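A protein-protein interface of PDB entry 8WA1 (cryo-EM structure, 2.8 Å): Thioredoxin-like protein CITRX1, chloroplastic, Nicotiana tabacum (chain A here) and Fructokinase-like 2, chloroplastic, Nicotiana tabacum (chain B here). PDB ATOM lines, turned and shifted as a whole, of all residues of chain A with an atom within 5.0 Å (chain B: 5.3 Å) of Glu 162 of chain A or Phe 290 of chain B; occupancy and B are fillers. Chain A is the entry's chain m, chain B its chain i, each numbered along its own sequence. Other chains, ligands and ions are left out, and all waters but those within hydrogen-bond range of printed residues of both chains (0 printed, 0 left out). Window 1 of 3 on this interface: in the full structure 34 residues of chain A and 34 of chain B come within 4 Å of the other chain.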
ATOM      1  N   PRO A 103       0.812  32.813 -23.209  1.00  0.00           N
ATOM      2  CA  PRO A 103       0.243  32.173 -22.037  1.00  0.00           C
ATOM      3  C   PRO A 103      -0.241  33.180 -21.023  1.00  0.00           C
ATOM      4  O   PRO A 103      -1.244  32.954 -20.367  1.00  0.00           O
ATOM      5  CB  PRO A 103       1.411  31.394 -21.490  1.00  0.00           C
ATOM      6  CG  PRO A 103       2.164  30.987 -22.696  1.00  0.00           C
ATOM      7  CD  PRO A 103       2.071  32.164 -23.613  1.00  0.00           C
ATOM      8  N   ARG A 142      12.173  33.733 -13.707  1.00  0.00           N
ATOM      9  CA  ARG A 142      12.847  32.917 -14.712  1.00  0.00           C
ATOM     10  C   ARG A 142      12.023  32.815 -15.990  1.00  0.00           C
ATOM     11  O   ARG A 142      12.573  32.581 -17.071  1.00  0.00           O
ATOM     12  CB  ARG A 142      13.143  31.532 -14.139  1.00  0.00           C
ATOM     13  CG  ARG A 142      13.828  31.586 -12.785  1.00  0.00           C
ATOM     14  CD  ARG A 142      14.467  30.260 -12.423  1.00  0.00           C
ATOM     15  NE  ARG A 142      13.490  29.178 -12.351  1.00  0.00           N
ATOM     16  CZ  ARG A 142      13.797  27.916 -12.075  1.00  0.00           C
ATOM     17  NH1 ARG A 142      15.056  27.572 -11.845  1.00  0.00           N
ATOM     18  NH2 ARG A 142      12.843  26.996 -12.029  1.00  0.00           N
ATOM     19  N   GLY A 143      10.718  33.006 -15.901  1.00  0.00           N
ATOM     20  CA  GLY A 143       9.885  32.848 -17.073  1.00  0.00           C
ATOM     21  C   GLY A 143       8.652  33.693 -17.064  1.00  0.00           C
ATOM     22  O   GLY A 143       8.269  34.220 -16.041  1.00  0.00           O
ATOM     23  N   LEU A 144       8.046  33.871 -18.218  1.00  0.00           N
ATOM     24  CA  LEU A 144       6.907  34.763 -18.278  1.00  0.00           C
ATOM     25  C   LEU A 144       5.607  34.402 -17.585  1.00  0.00           C
ATOM     26  O   LEU A 144       4.999  35.251 -16.954  1.00  0.00           O
ATOM     27  CB  LEU A 144       6.665  35.260 -19.691  1.00  0.00           C
ATOM     28  CG  LEU A 144       7.307  36.624 -19.948  1.00  0.00           C
ATOM     29  CD1 LEU A 144       6.875  37.590 -18.859  1.00  0.00           C
ATOM     30  CD2 LEU A 144       8.824  36.529 -19.983  1.00  0.00           C
ATOM     31  N   PRO A 145       5.160  33.152 -17.685  1.00  0.00           N
ATOM     32  CA  PRO A 145       3.900  32.926 -16.972  1.00  0.00           C
ATOM     33  C   PRO A 145       4.157  32.543 -15.520  1.00  0.00           C
ATOM     34  O   PRO A 145       3.916  31.401 -15.165  1.00  0.00           O
ATOM     35  CB  PRO A 145       3.248  31.799 -17.758  1.00  0.00           C
ATOM     36  CG  PRO A 145       4.070  31.642 -18.998  1.00  0.00           C
ATOM     37  CD  PRO A 145       5.445  32.065 -18.625  1.00  0.00           C
ATOM     38  N   THR A 146       4.613  33.472 -14.691  1.00  0.00           N
ATOM     39  CA  THR A 146       4.946  33.235 -13.293  1.00  0.00           C
ATOM     40  C   THR A 146       3.990  33.997 -12.385  1.00  0.00           C
ATOM     41  O   THR A 146       3.533  35.093 -12.725  1.00  0.00           O
ATOM     42  CB  THR A 146       6.389  33.651 -12.995  1.00  0.00           C
ATOM     43  OG1 THR A 146       6.662  34.916 -13.611  1.00  0.00           O
ATOM     44  CG2 THR A 146       7.362  32.609 -13.522  1.00  0.00           C
ATOM     45  N   ARG A 160       6.171  30.836  -5.355  1.00  0.00           N
ATOM     46  CA  ARG A 160       6.330  31.180  -6.762  1.00  0.00           C
ATOM     47  C   ARG A 160       5.913  29.986  -7.610  1.00  0.00           C
ATOM     48  O   ARG A 160       6.411  28.874  -7.408  1.00  0.00           O
ATOM     49  CB  ARG A 160       7.771  31.582  -7.073  1.00  0.00           C
ATOM     50  CG  ARG A 160       7.987  32.020  -8.514  1.00  0.00           C
ATOM     51  CD  ARG A 160       9.454  32.301  -8.802  1.00  0.00           C
ATOM     52  NE  ARG A 160      10.271  31.095  -8.717  1.00  0.00           N
ATOM     53  CZ  ARG A 160      11.577  31.059  -8.960  1.00  0.00           C
ATOM     54  NH1 ARG A 160      12.219  32.167  -9.304  1.00  0.00           N
ATOM     55  NH2 ARG A 160      12.242  29.917  -8.859  1.00  0.00           N
ATOM     56  N   THR A 161       5.004  30.218  -8.552  1.00  0.00           N
ATOM     57  CA  THR A 161       4.524  29.188  -9.464  1.00  0.00           C
ATOM     58  C   THR A 161       4.877  29.589 -10.889  1.00  0.00           C
ATOM     59  O   THR A 161       4.471  30.659 -11.356  1.00  0.00           O
ATOM     60  CB  THR A 161       3.016  28.982  -9.321  1.00  0.00           C
ATOM     61  OG1 THR A 161       2.334  30.208  -9.613  1.00  0.00           O
ATOM     62  CG2 THR A 161       2.671  28.540  -7.908  1.00  0.00           C
ATOM     63  N   GLU A 162       5.626  28.730 -11.576  1.00  0.00           N
ATOM     64  CA  GLU A 162       6.087  28.987 -12.933  1.00  0.00           C
ATOM     65  C   GLU A 162       5.250  28.179 -13.916  1.00  0.00           C
ATOM     66  O   GLU A 162       5.070  26.970 -13.738  1.00  0.00           O
ATOM     67  CB  GLU A 162       7.567  28.628 -13.084  1.00  0.00           C
ATOM     68  CG  GLU A 162       8.470  29.227 -12.019  1.00  0.00           C
ATOM     69  CD  GLU A 162       9.922  28.834 -12.203  1.00  0.00           C
ATOM     70  OE1 GLU A 162      10.276  28.363 -13.304  1.00  0.00           O
ATOM     71  OE2 GLU A 162      10.710  28.993 -11.246  1.00  0.00           O
ATOM     72  N   GLY A 163       4.745  28.846 -14.943  1.00  0.00           N
ATOM     73  CA  GLY A 163       3.966  28.203 -15.978  1.00  0.00           C
ATOM     74  C   GLY A 163       2.471  28.336 -15.732  1.00  0.00           C
ATOM     75  O   GLY A 163       2.013  28.692 -14.642  1.00  0.00           O
ATOM     76  N   LEU A 164       1.702  28.043 -16.778  1.00  0.00           N
ATOM     77  CA  LEU A 164       0.251  28.084 -16.668  1.00  0.00           C
ATOM     78  C   LEU A 164      -0.231  26.976 -15.742  1.00  0.00           C
ATOM     79  O   LEU A 164       0.144  25.810 -15.891  1.00  0.00           O
ATOM     80  CB  LEU A 164      -0.388  27.945 -18.051  1.00  0.00           C
ATOM     81  CG  LEU A 164      -1.834  28.421 -18.187  1.00  0.00           C
ATOM     82  CD1 LEU A 164      -1.942  29.908 -17.884  1.00  0.00           C
ATOM     83  CD2 LEU A 164      -2.375  28.112 -19.575  1.00  0.00           C
ATOM     84  N   ILE A 165      -1.071  27.344 -14.779  1.00  0.00           N
ATOM     85  CA  ILE A 165      -1.483  26.422 -13.725  1.00  0.00           C
ATOM     86  C   ILE A 165      -3.001  26.433 -13.590  1.00  0.00           C
ATOM     87  O   ILE A 165      -3.645  27.443 -13.908  1.00  0.00           O
ATOM     88  CB  ILE A 165      -0.807  26.775 -12.391  1.00  0.00           C
ATOM     89  CG1 ILE A 165      -1.054  28.244 -12.045  1.00  0.00           C
ATOM     90  CG2 ILE A 165       0.683  26.478 -12.453  1.00  0.00           C
ATOM     91  CD1 ILE A 165      -0.388  28.687 -10.764  1.00  0.00           C
ATOM     92  N   GLN B 287       6.739  21.435 -18.157  1.00  0.00           N
ATOM     93  CA  GLN B 287       5.933  22.581 -17.768  1.00  0.00           C
ATOM     94  C   GLN B 287       4.854  22.804 -18.818  1.00  0.00           C
ATOM     95  O   GLN B 287       4.975  22.364 -19.963  1.00  0.00           O
ATOM     96  CB  GLN B 287       6.790  23.841 -17.589  1.00  0.00           C
ATOM     97  CG  GLN B 287       7.641  23.835 -16.328  1.00  0.00           C
ATOM     98  CD  GLN B 287       8.647  24.963 -16.295  1.00  0.00           C
ATOM     99  OE1 GLN B 287       8.969  25.496 -15.234  1.00  0.00           O
ATOM    100  NE2 GLN B 287       9.158  25.330 -17.464  1.00  0.00           N
ATOM    101  N   HIS B 288       3.789  23.489 -18.411  1.00  0.00           N
ATOM    102  CA  HIS B 288       2.647  23.760 -19.272  1.00  0.00           C
ATOM    103  C   HIS B 288       2.598  25.243 -19.611  1.00  0.00           C
ATOM    104  O   HIS B 288       2.442  26.082 -18.717  1.00  0.00           O
ATOM    105  CB  HIS B 288       1.344  23.328 -18.594  1.00  0.00           C
ATOM    106  CG  HIS B 288       0.122  23.576 -19.422  1.00  0.00           C
ATOM    107  ND1 HIS B 288      -0.091  22.962 -20.637  1.00  0.00           N
ATOM    108  CD2 HIS B 288      -0.949  24.375 -19.211  1.00  0.00           C
ATOM    109  CE1 HIS B 288      -1.244  23.370 -21.137  1.00  0.00           C
ATOM    110  NE2 HIS B 288      -1.784  24.228 -20.291  1.00  0.00           N
ATOM    111  N   ALA B 289       2.721  25.553 -20.900  1.00  0.00           N
ATOM    112  CA  ALA B 289       2.648  26.920 -21.421  1.00  0.00           C
ATOM    113  C   ALA B 289       3.634  27.840 -20.695  1.00  0.00           C
ATOM    114  O   ALA B 289       3.265  28.808 -20.032  1.00  0.00           O
ATOM    115  CB  ALA B 289       1.218  27.459 -21.327  1.00  0.00           C
ATOM    116  N   PHE B 290       4.912  27.505 -20.849  1.00  0.00           N
ATOM    117  CA  PHE B 290       6.000  28.238 -20.219  1.00  0.00           C
ATOM    118  C   PHE B 290       6.856  28.893 -21.292  1.00  0.00           C
ATOM    119  O   PHE B 290       7.167  28.268 -22.312  1.00  0.00           O
ATOM    120  CB  PHE B 290       6.857  27.314 -19.348  1.00  0.00           C
ATOM    121  CG  PHE B 290       7.903  28.035 -18.546  1.00  0.00           C
ATOM    122  CD1 PHE B 290       7.593  28.572 -17.308  1.00  0.00           C
ATOM    123  CD2 PHE B 290       9.194  28.172 -19.028  1.00  0.00           C
ATOM    124  CE1 PHE B 290       8.551  29.235 -16.565  1.00  0.00           C
ATOM    125  CE2 PHE B 290      10.157  28.834 -18.289  1.00  0.00           C
ATOM    126  CZ  PHE B 290       9.834  29.365 -17.057  1.00  0.00           C
ATOM    127  N   VAL B 291       7.234  30.150 -21.058  1.00  0.00           N
ATOM    128  CA  VAL B 291       8.060  30.913 -21.981  1.00  0.00           C
ATOM    129  C   VAL B 291       9.327  31.331 -21.248  1.00  0.00           C
ATOM    130  O   VAL B 291       9.253  32.059 -20.254  1.00  0.00           O
ATOM    131  CB  VAL B 291       7.333  32.151 -22.535  1.00  0.00           C
ATOM    132  CG1 VAL B 291       8.257  32.947 -23.442  1.00  0.00           C
ATOM    133  CG2 VAL B 291       6.070  31.741 -23.275  1.00  0.00           C
ATOM    134  N   PRO B 292      10.512  30.897 -21.685  1.00  0.00           N
ATOM    135  CA  PRO B 292      11.739  31.319 -20.985  1.00  0.00           C
ATOM    136  C   PRO B 292      12.004  32.811 -21.091  1.00  0.00           C
ATOM    137  O   PRO B 292      12.208  33.477 -20.068  1.00  0.00           O
ATOM    138  CB  PRO B 292      12.834  30.487 -21.674  1.00  0.00           C
ATOM    139  CG  PRO B 292      12.107  29.350 -22.331  1.00  0.00           C
ATOM    140  CD  PRO B 292      10.787  29.912 -22.744  1.00  0.00           C
ATOM    141  N   GLY B 324      11.916  29.230 -27.609  1.00  0.00           N
ATOM    142  CA  GLY B 324      11.288  27.927 -27.605  1.00  0.00           C
ATOM    143  C   GLY B 324      10.362  27.791 -26.414  1.00  0.00           C
ATOM    144  O   GLY B 324      10.028  28.772 -25.746  1.00  0.00           O
ATOM    145  N   GLY B 325       9.951  26.550 -26.166  1.00  0.00           N
ATOM    146  CA  GLY B 325       9.098  26.255 -25.032  1.00  0.00           C
ATOM    147  C   GLY B 325       9.831  25.515 -23.934  1.00  0.00           C
ATOM    148  O   GLY B 325      10.703  26.080 -23.267  1.00  0.00           O
ATOM    149  N   CYS B 326       9.483  24.247 -23.738  1.00  0.00           N
ATOM    150  CA  CYS B 326      10.145  23.388 -22.770  1.00  0.00           C
ATOM    151  C   CYS B 326      10.518  22.073 -23.440  1.00  0.00           C
ATOM    152  O   CYS B 326      10.091  21.781 -24.561  1.00  0.00           O
ATOM    153  CB  CYS B 326       9.257  23.124 -21.546  1.00  0.00           C
ATOM    154  SG  CYS B 326       7.702  22.281 -21.917  1.00  0.00           S
ATOM    155  N   ALA B 379       5.163  22.519  -9.342  1.00  0.00           N
ATOM    156  CA  ALA B 379       5.468  23.868  -9.803  1.00  0.00           C
ATOM    157  C   ALA B 379       5.454  24.902  -8.684  1.00  0.00           C
ATOM    158  O   ALA B 379       5.302  26.097  -8.964  1.00  0.00           O
ATOM    159  CB  ALA B 379       4.491  24.284 -10.906  1.00  0.00           C
ATOM    160  N   THR B 381       7.486  26.827  -5.875  1.00  0.00           N
ATOM    161  CA  THR B 381       8.848  27.182  -5.486  1.00  0.00           C
ATOM    162  C   THR B 381       8.769  28.111  -4.279  1.00  0.00           C
ATOM    163  O   THR B 381       8.543  29.316  -4.429  1.00  0.00           O
ATOM    164  CB  THR B 381       9.598  27.847  -6.638  1.00  0.00           C
ATOM    165  OG1 THR B 381       9.400  27.095  -7.841  1.00  0.00           O
ATOM    166  CG2 THR B 381      11.087  27.916  -6.331  1.00  0.00           C
ATOM    167  N   SER B 399      11.243  23.310  -6.549  1.00  0.00           N
ATOM    168  CA  SER B 399       9.960  22.888  -7.098  1.00  0.00           C
ATOM    169  C   SER B 399      10.036  21.556  -7.841  1.00  0.00           C
ATOM    170  O   SER B 399       9.258  21.338  -8.777  1.00  0.00           O
ATOM    171  CB  SER B 399       9.407  23.969  -8.026  1.00  0.00           C
ATOM    172  OG  SER B 399      10.334  24.288  -9.050  1.00  0.00           O
ATOM    173  N   PHE B 425      17.583  26.435 -19.235  1.00  0.00           N
ATOM    174  CA  PHE B 425      16.717  26.671 -18.084  1.00  0.00           C
ATOM    175  C   PHE B 425      17.054  25.729 -16.934  1.00  0.00           C
ATOM    176  O   PHE B 425      16.871  26.078 -15.762  1.00  0.00           O
ATOM    177  CB  PHE B 425      15.251  26.517 -18.497  1.00  0.00           C
ATOM    178  CG  PHE B 425      14.276  26.765 -17.382  1.00  0.00           C
ATOM    179  CD1 PHE B 425      13.933  28.056 -17.018  1.00  0.00           C
ATOM    180  CD2 PHE B 425      13.696  25.706 -16.705  1.00  0.00           C
ATOM    181  CE1 PHE B 425      13.035  28.286 -15.995  1.00  0.00           C
ATOM    182  CE2 PHE B 425      12.796  25.930 -15.681  1.00  0.00           C
ATOM    183  CZ  PHE B 425      12.464  27.222 -15.326  1.00  0.00           C
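Of the 12 printed residues of chain A, 10 touch a printed residue of chain B. Of the 13 printed residues of chain B, 9 touch a printed residue of chain A. Printed residues of chain B that touch a printed residue of chain A: Gln 287, His 288, Ala 289, Phe 290, Val 291, Pro 292, Ala 379, Thr 381 and Phe 425. Hydrophobic or aromatic side chains of chain B that line the printed part of chain A: His 288, Ala 289, Phe 290, Ala 379 and Phe 425. Among the printed residues, no Asp or Glu carboxylate lies within 4 Å of a Lys or Arg side-chain nitrogen of the other chain.
Pro 103 of chain A touches Ala 289 of chain B (CB to O, 3.5 Å). Phe 425 of chain B touches Arg 142 of chain A (CZ to NH2, 3.3 Å). O of Val 291 of chain B touches CA of Gly 143 of chain A, 3.3 Å away. Gly 143 of chain A touches Pro 292 of chain B (CA to O, 3.8 Å). Pro 145 of chain A touches Ala 289 of chain B (CG to O, 3.1 Å). Pro 145 of chain A touches Val 291 of chain B. OE1 of Gln 287 of chain B touches OE1 of Glu 162 of chain A, at 3.7 Å. Glu 162 of chain A touches Phe 290 of chain B. Glu 162 of chain A touches Phe 425 of chain B (OE1 to CZ, 3.2 Å). Phe 290 of chain B touches Gly 163 of chain A (CD1 to N, 3.7 Å).
Glu 162 of chain A touches just these residues of chain B: Gln 287 (3.7 Å), Phe 290 (3.7 Å), Ala 379 (3.7 Å) and Phe 425 (3.2 Å). Printed residues of chain A within 4 Å of Phe 290 of chain B: Gly 143 (3.5 Å), Glu 162 (3.7 Å) and Gly 163 (3.7 Å). Printed residues of chain A within 4 Å of Ala 379 of chain B: Arg 160 (3.4 Å), Thr 161 (3.2 Å) and Glu 162 (3.7 Å). Of the printed residues of chain B, Leu 164 of chain A touches His 288 and Ala 289. Of the printed residues of chain B, Arg 160 of chain A touches Ala 379 (3.4 Å) and Thr 381 (2.8 Å). Printed residues of chain A within 4 Å of Pro 292 of chain B: Arg 142 and Gly 143. Gly 324 of chain B touches none of the printed residues of chain A. The nearest residue of chain A that does not touch Phe 290 of chain B is Pro 145 of chain A (4.1 Å).
The side-chain carboxylate of Glu 162 of chain A is in salt-bridge range of the guanidinium group of Arg 142 of chain A, 3.0 Å away. The backbone carbonyl oxygen (O) of Gly 143 of chain A is in hydrogen-bond range of the side-chain hydroxyl (OG1) of Thr 146 of chain A, at 3.0 Å. N of Gly 163 of chain A sits at hydrogen-bond distance from O of Pro 145 of chain A (2.7 Å). OE2 of Glu 162 of chain A is in salt-bridge range of NH2 of Arg 160 of chain A, 3.0 Å away. The side-chain sulfur (SG) of Cys 326 of chain B is in hydrogen-bond range of the backbone carbonyl oxygen (O) of Gln 287 of chain B. The side-chain hydroxyl (OG1) of Thr 381 of chain B lies close to the side-chain hydroxyl (OG) of Ser 399 of chain B (3.2 Å).
The backbone NH (N) of Leu 144 of chain A is in hydrogen-bond range of the backbone carbonyl oxygen (O) of Val 291 of chain B, at 3.0 Å. The backbone NH (N) of Thr 381 of chain B is in hydrogen-bond range of the backbone carbonyl oxygen (O) of Arg 160 of chain A (2.8 Å). N of Leu 164 of chain A is in hydrogen-bond range of O of His 288 of chain B. O of Arg 142 of chain A lies close to O of Pro 292 of chain B (3.1 Å). The backbone carbonyl oxygen (O) of Ala 379 of chain B sits close to the backbone carbonyl oxygen (O) of Arg 160 of chain A, at 3.4 Å.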
